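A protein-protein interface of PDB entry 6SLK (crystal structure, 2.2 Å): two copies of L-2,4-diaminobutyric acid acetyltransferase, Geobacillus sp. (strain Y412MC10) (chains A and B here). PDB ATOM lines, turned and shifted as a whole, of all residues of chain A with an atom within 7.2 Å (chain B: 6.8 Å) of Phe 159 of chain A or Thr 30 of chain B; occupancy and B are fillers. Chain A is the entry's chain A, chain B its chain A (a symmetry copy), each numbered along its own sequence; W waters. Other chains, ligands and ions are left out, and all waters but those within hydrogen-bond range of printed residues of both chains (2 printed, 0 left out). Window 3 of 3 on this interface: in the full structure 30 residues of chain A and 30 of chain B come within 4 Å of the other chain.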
ATOM      1  N   ASP A  43     -36.129 -38.713  10.738  1.00  0.00           N
ATOM      2  CA  ASP A  43     -35.486 -37.782  11.709  1.00  0.00           C
ATOM      3  C   ASP A  43     -36.154 -38.048  13.091  1.00  0.00           C
ATOM      4  O   ASP A  43     -37.375 -37.872  13.277  1.00  0.00           O
ATOM      5  CB  ASP A  43     -35.879 -36.330  11.350  1.00  0.00           C
ATOM      6  CG  ASP A  43     -35.253 -35.818  10.018  1.00  0.00           C
ATOM      7  OD1 ASP A  43     -34.269 -36.396   9.552  1.00  0.00           O
ATOM      8  OD2 ASP A  43     -35.774 -34.842   9.428  1.00  0.00           O
ATOM      9  N   TYR A 154     -35.457 -26.553   2.290  1.00  0.00           N
ATOM     10  CA  TYR A 154     -34.145 -26.533   2.954  1.00  0.00           C
ATOM     11  C   TYR A 154     -33.231 -27.383   2.068  1.00  0.00           C
ATOM     12  O   TYR A 154     -33.632 -28.451   1.577  1.00  0.00           O
ATOM     13  CB  TYR A 154     -34.178 -27.084   4.429  1.00  0.00           C
ATOM     14  CG  TYR A 154     -35.205 -26.460   5.372  1.00  0.00           C
ATOM     15  CD1 TYR A 154     -35.337 -25.073   5.493  1.00  0.00           C
ATOM     16  CD2 TYR A 154     -36.043 -27.259   6.161  1.00  0.00           C
ATOM     17  CE1 TYR A 154     -36.339 -24.521   6.294  1.00  0.00           C
ATOM     18  CE2 TYR A 154     -37.019 -26.700   7.007  1.00  0.00           C
ATOM     19  CZ  TYR A 154     -37.154 -25.353   7.086  1.00  0.00           C
ATOM     20  OH  TYR A 154     -38.162 -24.812   7.875  1.00  0.00           O
ATOM     21  N   GLY A 155     -31.997 -26.947   1.916  1.00  0.00           N
ATOM     22  CA  GLY A 155     -30.982 -27.733   1.177  1.00  0.00           C
ATOM     23  C   GLY A 155     -30.211 -28.672   2.088  1.00  0.00           C
ATOM     24  O   GLY A 155     -30.006 -28.342   3.288  1.00  0.00           O
ATOM     25  N   ALA A 156     -29.760 -29.807   1.523  1.00  0.00           N
ATOM     26  CA  ALA A 156     -28.850 -30.758   2.199  1.00  0.00           C
ATOM     27  C   ALA A 156     -27.649 -30.123   2.950  1.00  0.00           C
ATOM     28  O   ALA A 156     -27.255 -30.633   3.987  1.00  0.00           O
ATOM     29  CB  ALA A 156     -28.361 -31.870   1.228  1.00  0.00           C
ATOM     30  N   GLU A 157     -27.101 -29.037   2.427  1.00  0.00           N
ATOM     31  CA  GLU A 157     -25.912 -28.386   2.969  1.00  0.00           C
ATOM     32  C   GLU A 157     -26.187 -27.638   4.286  1.00  0.00           C
ATOM     33  O   GLU A 157     -25.278 -27.298   5.006  1.00  0.00           O
ATOM     34  CB  GLU A 157     -25.317 -27.399   1.929  1.00  0.00           C
ATOM     35  CG  GLU A 157     -26.194 -26.160   1.628  1.00  0.00           C
ATOM     36  CD  GLU A 157     -27.383 -26.412   0.647  1.00  0.00           C
ATOM     37  OE1 GLU A 157     -27.571 -27.540   0.026  1.00  0.00           O
ATOM     38  OE2 GLU A 157     -28.179 -25.444   0.521  1.00  0.00           O
ATOM     39  N   MET A 158     -27.440 -27.349   4.574  1.00  0.00           N
ATOM     40  CA  MET A 158     -27.810 -26.743   5.829  1.00  0.00           C
ATOM     41  C   MET A 158     -27.714 -27.726   7.026  1.00  0.00           C
ATOM     42  O   MET A 158     -27.842 -27.288   8.148  1.00  0.00           O
ATOM     43  CB  MET A 158     -29.267 -26.255   5.767  1.00  0.00           C
ATOM     44  CG  MET A 158     -29.501 -25.074   4.849  1.00  0.00           C
ATOM     45  SD  MET A 158     -31.275 -24.629   4.789  1.00  0.00           S
ATOM     46  CE  MET A 158     -31.648 -24.287   6.522  1.00  0.00           C
ATOM     47  N   PHE A 159     -27.616 -29.028   6.749  1.00  0.00           N
ATOM     48  CA  PHE A 159     -27.506 -30.073   7.750  1.00  0.00           C
ATOM     49  C   PHE A 159     -26.048 -30.222   8.277  1.00  0.00           C
ATOM     50  O   PHE A 159     -25.124 -29.634   7.712  1.00  0.00           O
ATOM     51  CB  PHE A 159     -28.117 -31.374   7.239  1.00  0.00           C
ATOM     52  CG  PHE A 159     -29.601 -31.266   7.092  1.00  0.00           C
ATOM     53  CD1 PHE A 159     -30.162 -30.629   5.986  1.00  0.00           C
ATOM     54  CD2 PHE A 159     -30.447 -31.731   8.085  1.00  0.00           C
ATOM     55  CE1 PHE A 159     -31.530 -30.477   5.861  1.00  0.00           C
ATOM     56  CE2 PHE A 159     -31.821 -31.588   7.960  1.00  0.00           C
ATOM     57  CZ  PHE A 159     -32.366 -30.960   6.842  1.00  0.00           C
ATOM     58  N   PRO A 160     -25.874 -30.916   9.416  1.00  0.00           N
ATOM     59  CA  PRO A 160     -24.559 -30.947  10.049  1.00  0.00           C
ATOM     60  C   PRO A 160     -23.613 -31.856   9.309  1.00  0.00           C
ATOM     61  O   PRO A 160     -24.077 -32.845   8.716  1.00  0.00           O
ATOM     62  CB  PRO A 160     -24.861 -31.535  11.446  1.00  0.00           C
ATOM     63  CG  PRO A 160     -26.355 -31.489  11.610  1.00  0.00           C
ATOM     64  CD  PRO A 160     -26.857 -31.678  10.217  1.00  0.00           C
ATOM     65  N   ASP A 161     -22.311 -31.583   9.427  1.00  0.00           N
ATOM     66  CA  ASP A 161     -21.247 -32.312   8.662  1.00  0.00           C
ATOM     67  C   ASP A 161     -21.226 -33.852   8.819  1.00  0.00           C
ATOM     68  O   ASP A 161     -21.160 -34.575   7.797  1.00  0.00           O
ATOM     69  CB  ASP A 161     -19.847 -31.785   9.015  1.00  0.00           C
ATOM     70  CG  ASP A 161     -19.636 -30.319   8.642  1.00  0.00           C
ATOM     71  OD1 ASP A 161     -20.152 -29.847   7.608  1.00  0.00           O
ATOM     72  OD2 ASP A 161     -18.945 -29.625   9.403  1.00  0.00           O
ATOM     73  N   GLY A 162     -21.270 -34.334  10.074  1.00  0.00           N
ATOM     74  CA  GLY A 162     -21.239 -35.791  10.402  1.00  0.00           C
ATOM     75  C   GLY A 162     -22.173 -36.662   9.572  1.00  0.00           C
ATOM     76  O   GLY A 162     -21.742 -37.591   8.907  1.00  0.00           O
ATOM     77  N   THR A 163     -23.455 -36.309   9.572  1.00  0.00           N
ATOM     78  CA  THR A 163     -24.486 -36.995   8.769  1.00  0.00           C
ATOM     79  C   THR A 163     -24.495 -36.561   7.297  1.00  0.00           C
ATOM     80  O   THR A 163     -23.844 -35.593   6.908  1.00  0.00           O
ATOM     81  CB  THR A 163     -25.905 -36.754   9.355  1.00  0.00           C
ATOM     82  OG1 THR A 163     -26.096 -35.345   9.619  1.00  0.00           O
ATOM     83  CG2 THR A 163     -26.131 -37.616  10.644  1.00  0.00           C
ATOM     84  N   THR A 164     -25.216 -37.326   6.481  1.00  0.00           N
ATOM     85  CA  THR A 164     -25.589 -36.899   5.143  1.00  0.00           C
ATOM     86  C   THR A 164     -27.128 -36.985   5.062  1.00  0.00           C
ATOM     87  O   THR A 164     -27.722 -38.067   5.005  1.00  0.00           O
ATOM     88  CB  THR A 164     -24.903 -37.713   4.032  1.00  0.00           C
ATOM     89  OG1 THR A 164     -25.171 -39.098   4.255  1.00  0.00           O
ATOM     90  CG2 THR A 164     -23.365 -37.450   3.999  1.00  0.00           C
ATOM     91  N   HIS A 165     -27.732 -35.805   5.108  1.00  0.00           N
ATOM     92  CA  HIS A 165     -29.148 -35.602   5.066  1.00  0.00           C
ATOM     93  C   HIS A 165     -29.463 -35.069   3.640  1.00  0.00           C
ATOM     94  O   HIS A 165     -28.666 -34.341   3.019  1.00  0.00           O
ATOM     95  CB  HIS A 165     -29.553 -34.607   6.190  1.00  0.00           C
ATOM     96  CG  HIS A 165     -31.016 -34.614   6.518  1.00  0.00           C
ATOM     97  ND1 HIS A 165     -31.978 -34.118   5.645  1.00  0.00           N
ATOM     98  CD2 HIS A 165     -31.690 -35.005   7.631  1.00  0.00           C
ATOM     99  CE1 HIS A 165     -33.178 -34.231   6.186  1.00  0.00           C
ATOM    100  NE2 HIS A 165     -33.034 -34.755   7.397  1.00  0.00           N
ATOM    101  N   GLU A 166     -30.643 -35.416   3.154  1.00  0.00           N
ATOM    102  CA  GLU A 166     -31.157 -34.906   1.884  1.00  0.00           C
ATOM    103  C   GLU A 166     -31.768 -33.493   1.973  1.00  0.00           C
ATOM    104  O   GLU A 166     -32.005 -32.944   3.050  1.00  0.00           O
ATOM    105  CB  GLU A 166     -32.211 -35.879   1.392  1.00  0.00           C
ATOM    106  CG  GLU A 166     -31.691 -37.269   1.112  1.00  0.00           C
ATOM    107  CD  GLU A 166     -32.764 -38.204   0.571  1.00  0.00           C
ATOM    108  OE1 GLU A 166     -33.954 -38.141   0.955  1.00  0.00           O
ATOM    109  OE2 GLU A 166     -32.424 -39.030  -0.279  1.00  0.00           O
ATOM    110  N   ASP A 167     -32.027 -32.890   0.815  1.00  0.00           N
ATOM    111  CA  ASP A 167     -32.886 -31.720   0.721  1.00  0.00           C
ATOM    112  C   ASP A 167     -34.295 -31.939   1.347  1.00  0.00           C
ATOM    113  O   ASP A 167     -34.807 -33.081   1.477  1.00  0.00           O
ATOM    114  CB  ASP A 167     -33.165 -31.345  -0.758  1.00  0.00           C
ATOM    115  CG  ASP A 167     -31.917 -31.016  -1.577  1.00  0.00           C
ATOM    116  OD1 ASP A 167     -30.800 -30.790  -1.013  1.00  0.00           O
ATOM    117  OD2 ASP A 167     -32.103 -30.972  -2.814  1.00  0.00           O
ATOM    118  N   GLU A 168     -34.939 -30.821   1.660  1.00  0.00           N
ATOM    119  CA  GLU A 168     -36.313 -30.867   2.110  1.00  0.00           C
ATOM    120  C   GLU A 168     -37.075 -29.848   1.283  1.00  0.00           C
ATOM    121  O   GLU A 168     -37.271 -28.725   1.694  1.00  0.00           O
ATOM    122  CB  GLU A 168     -36.314 -30.575   3.615  1.00  0.00           C
ATOM    123  CG  GLU A 168     -35.706 -31.699   4.476  1.00  0.00           C
ATOM    124  CD  GLU A 168     -36.640 -32.874   4.789  1.00  0.00           C
ATOM    125  OE1 GLU A 168     -37.877 -32.789   4.798  1.00  0.00           O
ATOM    126  OE2 GLU A 168     -36.109 -33.957   5.014  1.00  0.00           O
ATOM    127  N   GLU B  25     -32.651 -18.054  13.033  1.00  0.00           N
ATOM    128  CA  GLU B  25     -33.144 -18.217  11.655  1.00  0.00           C
ATOM    129  C   GLU B  25     -33.006 -19.668  11.302  1.00  0.00           C
ATOM    130  O   GLU B  25     -32.234 -20.415  11.944  1.00  0.00           O
ATOM    131  CB  GLU B  25     -32.323 -17.330  10.667  1.00  0.00           C
ATOM    132  CG  GLU B  25     -32.457 -15.808  10.916  1.00  0.00           C
ATOM    133  CD  GLU B  25     -33.920 -15.287  10.989  1.00  0.00           C
ATOM    134  OE1 GLU B  25     -34.734 -15.612  10.078  1.00  0.00           O
ATOM    135  OE2 GLU B  25     -34.293 -14.521  11.946  1.00  0.00           O
ATOM    136  N   ALA B  26     -33.713 -20.103  10.266  1.00  0.00           N
ATOM    137  CA  ALA B  26     -33.630 -21.527   9.933  1.00  0.00           C
ATOM    138  C   ALA B  26     -32.203 -21.947   9.720  1.00  0.00           C
ATOM    139  O   ALA B  26     -31.840 -23.097  10.057  1.00  0.00           O
ATOM    140  CB  ALA B  26     -34.456 -21.869   8.703  1.00  0.00           C
ATOM    141  N   ARG B  27     -31.377 -21.051   9.149  1.00  0.00           N
ATOM    142  CA  ARG B  27     -29.976 -21.470   8.888  1.00  0.00           C
ATOM    143  C   ARG B  27     -29.121 -21.630  10.195  1.00  0.00           C
ATOM    144  O   ARG B  27     -28.085 -22.195  10.147  1.00  0.00           O
ATOM    145  CB  ARG B  27     -29.276 -20.584   7.838  1.00  0.00           C
ATOM    146  CG  ARG B  27     -28.625 -19.344   8.420  1.00  0.00           C
ATOM    147  CD  ARG B  27     -28.427 -18.170   7.449  1.00  0.00           C
ATOM    148  NE  ARG B  27     -28.802 -16.937   8.177  1.00  0.00           N
ATOM    149  CZ  ARG B  27     -29.960 -16.257   8.075  1.00  0.00           C
ATOM    150  NH1 ARG B  27     -30.912 -16.597   7.195  1.00  0.00           N
ATOM    151  NH2 ARG B  27     -30.163 -15.190   8.853  1.00  0.00           N
ATOM    152  N   ASP B  28     -29.612 -21.207  11.356  1.00  0.00           N
ATOM    153  CA  ASP B  28     -28.898 -21.457  12.623  1.00  0.00           C
ATOM    154  C   ASP B  28     -29.102 -22.849  13.138  1.00  0.00           C
ATOM    155  O   ASP B  28     -28.480 -23.243  14.100  1.00  0.00           O
ATOM    156  CB  ASP B  28     -29.378 -20.462  13.679  1.00  0.00           C
ATOM    157  CG  ASP B  28     -29.058 -19.005  13.318  1.00  0.00           C
ATOM    158  OD1 ASP B  28     -27.855 -18.771  13.073  1.00  0.00           O
ATOM    159  OD2 ASP B  28     -29.977 -18.114  13.374  1.00  0.00           O
ATOM    160  N   GLY B  29     -30.007 -23.598  12.506  1.00  0.00           N
ATOM    161  CA  GLY B  29     -30.503 -24.846  13.018  1.00  0.00           C
ATOM    162  C   GLY B  29     -29.367 -25.775  13.367  1.00  0.00           C
ATOM    163  O   GLY B  29     -29.400 -26.403  14.402  1.00  0.00           O
ATOM    164  N   THR B  30     -28.375 -25.864  12.498  1.00  0.00           N
ATOM    165  CA  THR B  30     -27.295 -26.817  12.665  1.00  0.00           C
ATOM    166  C   THR B  30     -26.359 -26.476  13.858  1.00  0.00           C
ATOM    167  O   THR B  30     -25.955 -27.357  14.614  1.00  0.00           O
ATOM    168  CB  THR B  30     -26.512 -26.988  11.325  1.00  0.00           C
ATOM    169  OG1 THR B  30     -27.210 -27.985  10.568  1.00  0.00           O
ATOM    170  CG2 THR B  30     -25.035 -27.496  11.533  1.00  0.00           C
ATOM    171  N   ARG B  31     -26.061 -25.210  14.010  1.00  0.00           N
ATOM    172  CA  ARG B  31     -25.205 -24.738  15.102  1.00  0.00           C
ATOM    173  C   ARG B  31     -25.947 -24.820  16.438  1.00  0.00           C
ATOM    174  O   ARG B  31     -25.343 -25.127  17.427  1.00  0.00           O
ATOM    175  CB  ARG B  31     -24.737 -23.295  14.818  1.00  0.00           C
ATOM    176  CG  ARG B  31     -23.494 -23.273  13.895  1.00  0.00           C
ATOM    177  CD  ARG B  31     -23.413 -22.014  13.043  1.00  0.00           C
ATOM    178  NE  ARG B  31     -23.038 -20.809  13.805  1.00  0.00           N
ATOM    179  CZ  ARG B  31     -23.777 -19.702  13.988  1.00  0.00           C
ATOM    180  NH1 ARG B  31     -25.022 -19.586  13.489  1.00  0.00           N
ATOM    181  NH2 ARG B  31     -23.269 -18.696  14.728  1.00  0.00           N
ATOM    182  N   VAL B  32     -27.265 -24.601  16.430  1.00  0.00           N
ATOM    183  CA  VAL B  32     -28.065 -24.779  17.621  1.00  0.00           C
ATOM    184  C   VAL B  32     -28.008 -26.252  18.000  1.00  0.00           C
ATOM    185  O   VAL B  32     -27.803 -26.587  19.151  1.00  0.00           O
ATOM    186  CB  VAL B  32     -29.494 -24.275  17.463  1.00  0.00           C
ATOM    187  CG1 VAL B  32     -30.393 -24.715  18.637  1.00  0.00           C
ATOM    188  CG2 VAL B  32     -29.473 -22.765  17.345  1.00  0.00           C
ATOM    189  N   TRP B  33     -28.171 -27.131  17.053  1.00  0.00           N
ATOM    190  CA  TRP B  33     -28.181 -28.552  17.355  1.00  0.00           C
ATOM    191  C   TRP B  33     -26.823 -28.954  17.905  1.00  0.00           C
ATOM    192  O   TRP B  33     -26.752 -29.829  18.758  1.00  0.00           O
ATOM    193  CB  TRP B  33     -28.459 -29.362  16.084  1.00  0.00           C
ATOM    194  CG  TRP B  33     -28.362 -30.882  16.207  1.00  0.00           C
ATOM    195  CD1 TRP B  33     -29.363 -31.737  16.581  1.00  0.00           C
ATOM    196  CD2 TRP B  33     -27.228 -31.689  15.928  1.00  0.00           C
ATOM    197  NE1 TRP B  33     -28.899 -33.052  16.597  1.00  0.00           N
ATOM    198  CE2 TRP B  33     -27.593 -33.038  16.169  1.00  0.00           C
ATOM    199  CE3 TRP B  33     -25.937 -31.407  15.493  1.00  0.00           C
ATOM    200  CZ2 TRP B  33     -26.733 -34.083  15.965  1.00  0.00           C
ATOM    201  CZ3 TRP B  33     -25.057 -32.477  15.274  1.00  0.00           C
ATOM    202  CH2 TRP B  33     -25.465 -33.789  15.518  1.00  0.00           C
ATOM    203  N   GLU B  34     -25.752 -28.365  17.363  1.00  0.00           N
ATOM    204  CA  GLU B  34     -24.397 -28.616  17.895  1.00  0.00           C
ATOM    205  C   GLU B  34     -24.185 -28.196  19.359  1.00  0.00           C
ATOM    206  O   GLU B  34     -23.669 -28.974  20.147  1.00  0.00           O
ATOM    207  CB  GLU B  34     -23.347 -27.955  17.021  1.00  0.00           C
ATOM    208  CG  GLU B  34     -22.999 -28.871  15.831  1.00  0.00           C
ATOM    209  CD  GLU B  34     -22.296 -28.185  14.646  1.00  0.00           C
ATOM    210  OE1 GLU B  34     -22.121 -26.946  14.607  1.00  0.00           O
ATOM    211  OE2 GLU B  34     -21.966 -28.925  13.723  1.00  0.00           O
ATOM    212  N   LEU B  35     -24.629 -26.981  19.678  1.00  0.00           N
ATOM    213  CA  LEU B  35     -24.648 -26.487  21.007  1.00  0.00           C
ATOM    214  C   LEU B  35     -25.385 -27.472  21.912  1.00  0.00           C
ATOM    215  O   LEU B  35     -24.800 -27.996  22.819  1.00  0.00           O
ATOM    216  CB  LEU B  35     -25.307 -25.142  21.006  1.00  0.00           C
ATOM    217  CG  LEU B  35     -25.408 -24.453  22.373  1.00  0.00           C
ATOM    218  CD1 LEU B  35     -24.114 -23.748  22.829  1.00  0.00           C
ATOM    219  CD2 LEU B  35     -26.584 -23.502  22.309  1.00  0.00           C
ATOM    220  N   PRO B  47     -31.705 -32.312  13.957  1.00  0.00           N
ATOM    221  CA  PRO B  47     -31.354 -31.015  13.377  1.00  0.00           C
ATOM    222  C   PRO B  47     -32.542 -30.268  12.695  1.00  0.00           C
ATOM    223  O   PRO B  47     -32.690 -29.059  12.856  1.00  0.00           O
ATOM    224  CB  PRO B  47     -30.196 -31.367  12.437  1.00  0.00           C
ATOM    225  CG  PRO B  47     -29.628 -32.689  12.941  1.00  0.00           C
ATOM    226  CD  PRO B  47     -30.809 -33.408  13.538  1.00  0.00           C
ATOM    227  N   TYR B  48     -33.388 -31.015  12.002  1.00  0.00           N
ATOM    228  CA  TYR B  48     -34.562 -30.489  11.393  1.00  0.00           C
ATOM    229  C   TYR B  48     -35.453 -29.732  12.384  1.00  0.00           C
ATOM    230  O   TYR B  48     -36.031 -28.654  12.060  1.00  0.00           O
ATOM    231  CB  TYR B  48     -35.355 -31.673  10.774  1.00  0.00           C
ATOM    232  CG  TYR B  48     -36.532 -31.249   9.907  1.00  0.00           C
ATOM    233  CD1 TYR B  48     -36.364 -30.805   8.584  1.00  0.00           C
ATOM    234  CD2 TYR B  48     -37.820 -31.284  10.414  1.00  0.00           C
ATOM    235  CE1 TYR B  48     -37.462 -30.400   7.814  1.00  0.00           C
ATOM    236  CE2 TYR B  48     -38.924 -30.933   9.654  1.00  0.00           C
ATOM    237  CZ  TYR B  48     -38.759 -30.471   8.365  1.00  0.00           C
ATOM    238  OH  TYR B  48     -39.923 -30.113   7.690  1.00  0.00           O
ATOM    239  N   TYR B  50     -34.586 -28.119  15.008  1.00  0.00           N
ATOM    240  CA  TYR B  50     -33.992 -26.807  15.310  1.00  0.00           C
ATOM    241  C   TYR B  50     -34.163 -25.810  14.156  1.00  0.00           C
ATOM    242  O   TYR B  50     -34.405 -24.567  14.371  1.00  0.00           O
ATOM    243  CB  TYR B  50     -32.541 -26.912  15.874  1.00  0.00           C
ATOM    244  CG  TYR B  50     -32.530 -27.685  17.179  1.00  0.00           C
ATOM    245  CD1 TYR B  50     -33.065 -27.134  18.343  1.00  0.00           C
ATOM    246  CD2 TYR B  50     -32.052 -28.982  17.244  1.00  0.00           C
ATOM    247  CE1 TYR B  50     -33.132 -27.875  19.529  1.00  0.00           C
ATOM    248  CE2 TYR B  50     -32.092 -29.721  18.411  1.00  0.00           C
ATOM    249  CZ  TYR B  50     -32.618 -29.172  19.574  1.00  0.00           C
ATOM    250  OH  TYR B  50     -32.669 -29.933  20.744  1.00  0.00           O
ATOM    251  N   MET B  51     -34.185 -26.356  12.951  1.00  0.00           N
ATOM    252  CA  MET B  51     -34.474 -25.518  11.755  1.00  0.00           C
ATOM    253  C   MET B  51     -35.904 -24.998  11.743  1.00  0.00           C
ATOM    254  O   MET B  51     -36.113 -23.811  11.475  1.00  0.00           O
ATOM    255  CB  MET B  51     -34.231 -26.294  10.473  1.00  0.00           C
ATOM    256  CG  MET B  51     -32.774 -26.532  10.140  1.00  0.00           C
ATOM    257  SD  MET B  51     -32.679 -27.644   8.681  1.00  0.00           S
ATOM    258  CE  MET B  51     -31.037 -28.292   9.010  1.00  0.00           C
HETATM  259  O   HOH W   1     -28.902 -25.008   9.739  1.00  0.00           O
HETATM  260  O   HOH W   2     -32.850 -33.667  10.930  1.00  0.00           O
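O of Met 158 of chain A is in hydrogen-bond range of OG1 of Thr 30 of chain B, at 2.6 Å.
The backbone nitrogen (N) of Pro 160 of chain A lies close to the side-chain hydroxyl (OG1) of Thr 30 of chain B, at 3.4 Å.
OD1 of Asp 43 of chain A is in hydrogen-bond range of NE2 of His 165 of chain A, 3.0 Å away.
The backbone carbonyl oxygen (O) of Tyr 154 of chain A lies within hydrogen-bond range of the backbone NH (N) of Glu 168 of chain A (2.7 Å).
N of Gly 155 of chain A lies within hydrogen-bond range of SD of Met 158 of chain A, at 3.8 Å.
The backbone carbonyl oxygen (O) of Pro 160 of chain A sits at hydrogen-bond distance from the side-chain hydroxyl (OG1) of Thr 163 of chain A (3.3 Å).
Asp 43 of chain A touches Tyr 48 of chain B (OD2 to CB, 3.5 Å).
Tyr 154 of chain A touches Tyr 48 of chain B.
O of Ala 26 of chain B touches CE of Met 158 of chain A, 3.7 Å away.
Met 51 of chain B touches Met 158 of chain A (CE to O, 3.5 Å).
Thr 30 of chain B touches Phe 159 of chain A.
CE2 of Phe 159 of chain A touches CE of Met 51 of chain B, 3.5 Å away.
CE3 of Trp 33 of chain B touches CG of Pro 160 of chain A, 3.9 Å away.
Pro 160 of chain A touches Pro 47 of chain B (CG to CG, 3.7 Å).
CE1 of Tyr 48 of chain B touches OE1 of Glu 168 of chain A (3.9 Å).
Phe 159 of chain A touches just these residues of chain B: Thr 30 and Met 51.
Of the printed residues of chain A, Pro 47 of chain B touches Pro 160.
Printed residues of chain B within 4 Å of Tyr 154 of chain A: Tyr 48.
Arg 31 of chain B touches none of the printed residues of chain A.
The nearest printed residue of chain B that does not touch Phe 159 of chain A is Tyr 48 of chain B (4.4 Å).
The nearest residue of chain A that does not touch Thr 30 of chain B is Asp 161 of chain A (5.3 Å).
The nearest printed residue of chain A that does not touch Met 51 of chain B is Tyr 154 of chain A (4.2 Å).
Of the 16 printed residues of chain A, 6 touch a printed residue of chain B.
Hydrophobic or aromatic side chains of chain B within 4 Å of the printed part of chain A: Trp 33, Pro 47, Tyr 48 and Met 51.
Among the printed residues, no Asp or Glu carboxylate lies within 4 Å of a Lys or Arg side-chain nitrogen of the other chain.
No position is printed for both chains.
Water W2 bridges N of Tyr 48 of chain B (2.9 Å) and OD1 of Asp 43 of chain A (3.4 Å).
Water W1 lies within hydrogen-bond range of N of Thr 30 of chain B, O of Arg 27 of chain B, O of Met 158 of chain A and N of Gly 29 of chain B.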
